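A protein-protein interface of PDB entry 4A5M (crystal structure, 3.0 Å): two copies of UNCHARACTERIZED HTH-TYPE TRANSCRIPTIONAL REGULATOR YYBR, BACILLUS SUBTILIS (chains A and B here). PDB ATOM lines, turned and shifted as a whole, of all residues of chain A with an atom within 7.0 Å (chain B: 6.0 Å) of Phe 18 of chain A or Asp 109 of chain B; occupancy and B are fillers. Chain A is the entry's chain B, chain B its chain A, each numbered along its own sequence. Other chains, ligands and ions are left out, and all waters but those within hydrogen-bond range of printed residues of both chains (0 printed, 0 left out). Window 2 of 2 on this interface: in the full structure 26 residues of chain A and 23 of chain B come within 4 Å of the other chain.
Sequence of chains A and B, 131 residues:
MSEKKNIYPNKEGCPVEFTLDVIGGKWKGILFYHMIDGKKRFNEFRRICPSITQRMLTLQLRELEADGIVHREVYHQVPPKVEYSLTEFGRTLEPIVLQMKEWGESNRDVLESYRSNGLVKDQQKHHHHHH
The backbone NH (N) of Gly 104 of chain B sits close to the side-chain hydroxyl (OG1) of Thr 19 of chain A, at 3.1 Å.
NE1 of Trp 103 of chain B lies close to ND2 of Asn 107 of chain B.
Among the printed residues, pairs that only touch across the chains: Pro 15 of chain A with Gly 104 of chain B (3.7 Å), Phe 18 of chain A with Asn 107 of chain B (3.5 Å), Phe 18 of chain A with Arg 108 of chain B (3.9 Å), Phe 18 of chain A with Asp 109 of chain B (3.7 Å), Thr 19 of chain A with Trp 103 of chain B (3.4 Å), Val 22 of chain A with Trp 103 of chain B (3.9 Å) and Phe 89 of chain A with Trp 103 of chain B (3.9 Å).
Phe 18 of chain A touches just these residues of chain B: Asn 107 (3.5 Å), Arg 108 (3.9 Å) and Asp 109 (3.7 Å). Printed residues of chain A within 4 Å of Trp 103 of chain B: Thr 19 (3.4 Å), Val 22 (3.9 Å) and Phe 89 (3.9 Å). Printed residues of chain A within 4 Å of Gly 104 of chain B: Pro 15 (3.7 Å) and Thr 19 (3.1 Å). Asp 109 of chain B touches one residue of chain A. The nearest printed residue of chain B that does not touch Phe 18 of chain A is Trp 103 of chain B (4.5 Å). The nearest printed residue of chain B that does not touch Thr 19 of chain A is Asn 107 of chain B (6.9 Å).
Hydrophobic or aromatic side chains of chain A that line the printed part of chain B: Phe 18, Val 22 and Phe 89. Of the 6 printed residues of chain B, 5 touch a printed residue of chain A. Printed residues of chain B that touch a printed residue of chain A: Trp 103, Gly 104, Asn 107, Arg 108 and Asp 109. Hydrophobic or aromatic side chains of chain B within 4 Å of the printed part of chain A: Trp 103. Among the printed residues, 8 pairs touch across the chains. Among the printed residues, no Asp or Glu carboxylate lies within 4 Å of a Lys or Arg side-chain nitrogen of the other chain.
No position is printed for both chains.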
ATOM      1  N   CYS A  14      -4.407 -19.787  36.580  1.00  0.00           N
ATOM      2  CA  CYS A  14      -3.512 -18.611  36.607  1.00  0.00           C
ATOM      3  C   CYS A  14      -3.284 -18.208  35.169  1.00  0.00           C
ATOM      4  O   CYS A  14      -2.294 -18.623  34.567  1.00  0.00           O
ATOM      5  CB  CYS A  14      -2.186 -18.969  37.276  1.00  0.00           C
ATOM      6  SG  CYS A  14      -2.355 -19.528  39.006  1.00  0.00           S
ATOM      7  N   PRO A  15      -4.218 -17.418  34.600  1.00  0.00           N
ATOM      8  CA  PRO A  15      -4.231 -17.112  33.157  1.00  0.00           C
ATOM      9  C   PRO A  15      -3.373 -15.922  32.689  1.00  0.00           C
ATOM     10  O   PRO A  15      -3.111 -15.799  31.487  1.00  0.00           O
ATOM     11  CB  PRO A  15      -5.714 -16.840  32.877  1.00  0.00           C
ATOM     12  CG  PRO A  15      -6.257 -16.328  34.170  1.00  0.00           C
ATOM     13  CD  PRO A  15      -5.400 -16.863  35.288  1.00  0.00           C
ATOM     14  N   VAL A  16      -2.960 -15.058  33.615  1.00  0.00           N
ATOM     15  CA  VAL A  16      -1.974 -14.006  33.316  1.00  0.00           C
ATOM     16  C   VAL A  16      -0.564 -14.607  33.225  1.00  0.00           C
ATOM     17  O   VAL A  16       0.308 -14.067  32.529  1.00  0.00           O
ATOM     18  CB  VAL A  16      -2.006 -12.872  34.375  1.00  0.00           C
ATOM     19  CG1 VAL A  16      -0.690 -12.118  34.420  1.00  0.00           C
ATOM     20  CG2 VAL A  16      -3.149 -11.904  34.104  1.00  0.00           C
ATOM     21  N   GLU A  17      -0.341 -15.716  33.931  1.00  0.00           N
ATOM     22  CA  GLU A  17       0.918 -16.451  33.847  1.00  0.00           C
ATOM     23  C   GLU A  17       1.279 -16.825  32.398  1.00  0.00           C
ATOM     24  O   GLU A  17       2.385 -16.498  31.929  1.00  0.00           O
ATOM     25  CB  GLU A  17       0.865 -17.695  34.739  1.00  0.00           C
ATOM     26  CG  GLU A  17       1.784 -18.821  34.295  1.00  0.00           C
ATOM     27  CD  GLU A  17       2.126 -19.748  35.429  1.00  0.00           C
ATOM     28  OE1 GLU A  17       1.359 -20.688  35.683  1.00  0.00           O
ATOM     29  OE2 GLU A  17       3.175 -19.530  36.059  1.00  0.00           O
ATOM     30  N   PHE A  18       0.347 -17.463  31.683  1.00  0.00           N
ATOM     31  CA  PHE A  18       0.609 -17.891  30.297  1.00  0.00           C
ATOM     32  C   PHE A  18       1.284 -16.727  29.585  1.00  0.00           C
ATOM     33  O   PHE A  18       2.368 -16.879  29.047  1.00  0.00           O
ATOM     34  CB  PHE A  18      -0.670 -18.264  29.536  1.00  0.00           C
ATOM     35  CG  PHE A  18      -0.447 -19.042  28.258  1.00  0.00           C
ATOM     36  CD1 PHE A  18       0.423 -18.597  27.259  1.00  0.00           C
ATOM     37  CD2 PHE A  18      -1.147 -20.229  28.042  1.00  0.00           C
ATOM     38  CE1 PHE A  18       0.594 -19.318  26.088  1.00  0.00           C
ATOM     39  CE2 PHE A  18      -0.973 -20.957  26.877  1.00  0.00           C
ATOM     40  CZ  PHE A  18      -0.100 -20.500  25.900  1.00  0.00           C
ATOM     41  N   THR A  19       0.636 -15.563  29.598  1.00  0.00           N
ATOM     42  CA  THR A  19       1.145 -14.379  28.916  1.00  0.00           C
ATOM     43  C   THR A  19       2.495 -13.951  29.452  1.00  0.00           C
ATOM     44  O   THR A  19       3.382 -13.606  28.683  1.00  0.00           O
ATOM     45  CB  THR A  19       0.182 -13.201  29.094  1.00  0.00           C
ATOM     46  OG1 THR A  19      -1.163 -13.668  28.979  1.00  0.00           O
ATOM     47  CG2 THR A  19       0.417 -12.115  28.057  1.00  0.00           C
ATOM     48  N   LEU A  20       2.654 -13.969  30.769  1.00  0.00           N
ATOM     49  CA  LEU A  20       3.897 -13.491  31.372  1.00  0.00           C
ATOM     50  C   LEU A  20       5.075 -14.392  31.052  1.00  0.00           C
ATOM     51  O   LEU A  20       6.166 -13.886  30.823  1.00  0.00           O
ATOM     52  CB  LEU A  20       3.760 -13.292  32.883  1.00  0.00           C
ATOM     53  CG  LEU A  20       3.317 -11.862  33.216  1.00  0.00           C
ATOM     54  CD1 LEU A  20       2.915 -11.734  34.675  1.00  0.00           C
ATOM     55  CD2 LEU A  20       4.393 -10.838  32.863  1.00  0.00           C
ATOM     56  N   ASP A  21       4.863 -15.708  31.004  1.00  0.00           N
ATOM     57  CA  ASP A  21       5.907 -16.626  30.511  1.00  0.00           C
ATOM     58  C   ASP A  21       6.348 -16.149  29.121  1.00  0.00           C
ATOM     59  O   ASP A  21       7.500 -15.767  28.907  1.00  0.00           O
ATOM     60  CB  ASP A  21       5.399 -18.079  30.414  1.00  0.00           C
ATOM     61  CG  ASP A  21       5.015 -18.678  31.775  1.00  0.00           C
ATOM     62  OD1 ASP A  21       5.786 -18.528  32.752  1.00  0.00           O
ATOM     63  OD2 ASP A  21       3.944 -19.325  31.848  1.00  0.00           O
ATOM     64  N   VAL A  22       5.385 -16.110  28.207  1.00  0.00           N
ATOM     65  CA  VAL A  22       5.606 -15.701  26.826  1.00  0.00           C
ATOM     66  C   VAL A  22       6.312 -14.335  26.698  1.00  0.00           C
ATOM     67  O   VAL A  22       7.352 -14.226  26.044  1.00  0.00           O
ATOM     68  CB  VAL A  22       4.238 -15.638  26.096  1.00  0.00           C
ATOM     69  CG1 VAL A  22       4.377 -15.095  24.679  1.00  0.00           C
ATOM     70  CG2 VAL A  22       3.541 -16.990  26.128  1.00  0.00           C
ATOM     71  N   ILE A  23       5.731 -13.310  27.319  1.00  0.00           N
ATOM     72  CA  ILE A  23       6.138 -11.913  27.102  1.00  0.00           C
ATOM     73  C   ILE A  23       6.716 -11.167  28.325  1.00  0.00           C
ATOM     74  O   ILE A  23       7.406 -10.152  28.172  1.00  0.00           O
ATOM     75  CB  ILE A  23       4.932 -11.127  26.527  1.00  0.00           C
ATOM     76  CG1 ILE A  23       5.431  -9.952  25.722  1.00  0.00           C
ATOM     77  CG2 ILE A  23       4.011 -10.652  27.641  1.00  0.00           C
ATOM     78  CD1 ILE A  23       6.257 -10.308  24.508  1.00  0.00           C
ATOM     79  N   GLY A  24       6.477 -11.687  29.525  1.00  0.00           N
ATOM     80  CA  GLY A  24       7.049 -11.103  30.720  1.00  0.00           C
ATOM     81  C   GLY A  24       8.548 -11.246  30.699  1.00  0.00           C
ATOM     82  O   GLY A  24       9.137 -11.722  29.720  1.00  0.00           O
ATOM     83  N   PHE A  89       1.349 -14.062  14.785  1.00  0.00           N
ATOM     84  CA  PHE A  89       0.953 -14.341  16.164  1.00  0.00           C
ATOM     85  C   PHE A  89       1.591 -13.356  17.122  1.00  0.00           C
ATOM     86  O   PHE A  89       0.912 -12.708  17.920  1.00  0.00           O
ATOM     87  CB  PHE A  89       1.434 -15.751  16.497  1.00  0.00           C
ATOM     88  CG  PHE A  89       1.108 -16.223  17.880  1.00  0.00           C
ATOM     89  CD1 PHE A  89       1.944 -15.923  18.947  1.00  0.00           C
ATOM     90  CD2 PHE A  89       0.004 -17.022  18.104  1.00  0.00           C
ATOM     91  CE1 PHE A  89       1.660 -16.386  20.220  1.00  0.00           C
ATOM     92  CE2 PHE A  89      -0.285 -17.493  19.375  1.00  0.00           C
ATOM     93  CZ  PHE A  89       0.546 -17.178  20.434  1.00  0.00           C
ATOM     94  N   TRP B 103      -5.439 -11.666  26.796  1.00  0.00           N
ATOM     95  CA  TRP B 103      -4.634 -12.286  25.753  1.00  0.00           C
ATOM     96  C   TRP B 103      -4.286 -13.699  26.112  1.00  0.00           C
ATOM     97  O   TRP B 103      -4.490 -14.602  25.309  1.00  0.00           O
ATOM     98  CB  TRP B 103      -3.385 -11.473  25.547  1.00  0.00           C
ATOM     99  CG  TRP B 103      -2.503 -11.927  24.423  1.00  0.00           C
ATOM    100  CD1 TRP B 103      -2.450 -11.423  23.128  1.00  0.00           C
ATOM    101  CD2 TRP B 103      -1.461 -12.965  24.471  1.00  0.00           C
ATOM    102  NE1 TRP B 103      -1.489 -12.073  22.392  1.00  0.00           N
ATOM    103  CE2 TRP B 103      -0.862 -13.008  23.140  1.00  0.00           C
ATOM    104  CE3 TRP B 103      -0.987 -13.830  25.445  1.00  0.00           C
ATOM    105  CZ2 TRP B 103       0.159 -13.894  22.822  1.00  0.00           C
ATOM    106  CZ3 TRP B 103       0.049 -14.712  25.114  1.00  0.00           C
ATOM    107  CH2 TRP B 103       0.610 -14.737  23.837  1.00  0.00           C
ATOM    108  N   GLY B 104      -3.766 -13.913  27.318  1.00  0.00           N
ATOM    109  CA  GLY B 104      -3.515 -15.266  27.828  1.00  0.00           C
ATOM    110  C   GLY B 104      -4.732 -16.186  27.751  1.00  0.00           C
ATOM    111  O   GLY B 104      -4.596 -17.398  27.608  1.00  0.00           O
ATOM    112  N   SER B 106      -7.478 -15.749  25.441  1.00  0.00           N
ATOM    113  CA  SER B 106      -7.695 -16.021  24.025  1.00  0.00           C
ATOM    114  C   SER B 106      -6.737 -17.111  23.557  1.00  0.00           C
ATOM    115  O   SER B 106      -7.156 -18.144  23.051  1.00  0.00           O
ATOM    116  CB  SER B 106      -7.458 -14.756  23.190  1.00  0.00           C
ATOM    117  OG  SER B 106      -8.305 -13.710  23.614  1.00  0.00           O
ATOM    118  N   ASN B 107      -5.449 -16.843  23.740  1.00  0.00           N
ATOM    119  CA  ASN B 107      -4.376 -17.613  23.139  1.00  0.00           C
ATOM    120  C   ASN B 107      -3.888 -18.720  24.054  1.00  0.00           C
ATOM    121  O   ASN B 107      -2.728 -18.726  24.484  1.00  0.00           O
ATOM    122  CB  ASN B 107      -3.217 -16.674  22.779  1.00  0.00           C
ATOM    123  CG  ASN B 107      -3.658 -15.520  21.894  1.00  0.00           C
ATOM    124  OD1 ASN B 107      -4.297 -15.715  20.871  1.00  0.00           O
ATOM    125  ND2 ASN B 107      -3.314 -14.310  22.292  1.00  0.00           N
ATOM    126  N   ARG B 108      -4.775 -19.665  24.337  1.00  0.00           N
ATOM    127  CA  ARG B 108      -4.421 -20.822  25.132  1.00  0.00           C
ATOM    128  C   ARG B 108      -4.047 -21.998  24.181  1.00  0.00           C
ATOM    129  O   ARG B 108      -4.887 -22.829  23.815  1.00  0.00           O
ATOM    130  CB  ARG B 108      -5.542 -21.160  26.151  1.00  0.00           C
ATOM    131  CG  ARG B 108      -4.984 -21.890  27.346  1.00  0.00           C
ATOM    132  CD  ARG B 108      -5.681 -21.977  28.721  1.00  0.00           C
ATOM    133  NE  ARG B 108      -6.934 -22.746  28.759  1.00  0.00           N
ATOM    134  CZ  ARG B 108      -7.101 -24.052  28.495  1.00  0.00           C
ATOM    135  NH1 ARG B 108      -6.094 -24.833  28.101  1.00  0.00           N
ATOM    136  NH2 ARG B 108      -8.321 -24.588  28.599  1.00  0.00           N
ATOM    137  N   ASP B 109      -2.770 -22.063  23.795  1.00  0.00           N
ATOM    138  CA  ASP B 109      -2.280 -23.001  22.773  1.00  0.00           C
ATOM    139  C   ASP B 109      -2.437 -22.382  21.386  1.00  0.00           C
ATOM    140  O   ASP B 109      -1.622 -22.615  20.496  1.00  0.00           O
ATOM    141  CB  ASP B 109      -3.008 -24.348  22.846  1.00  0.00           C
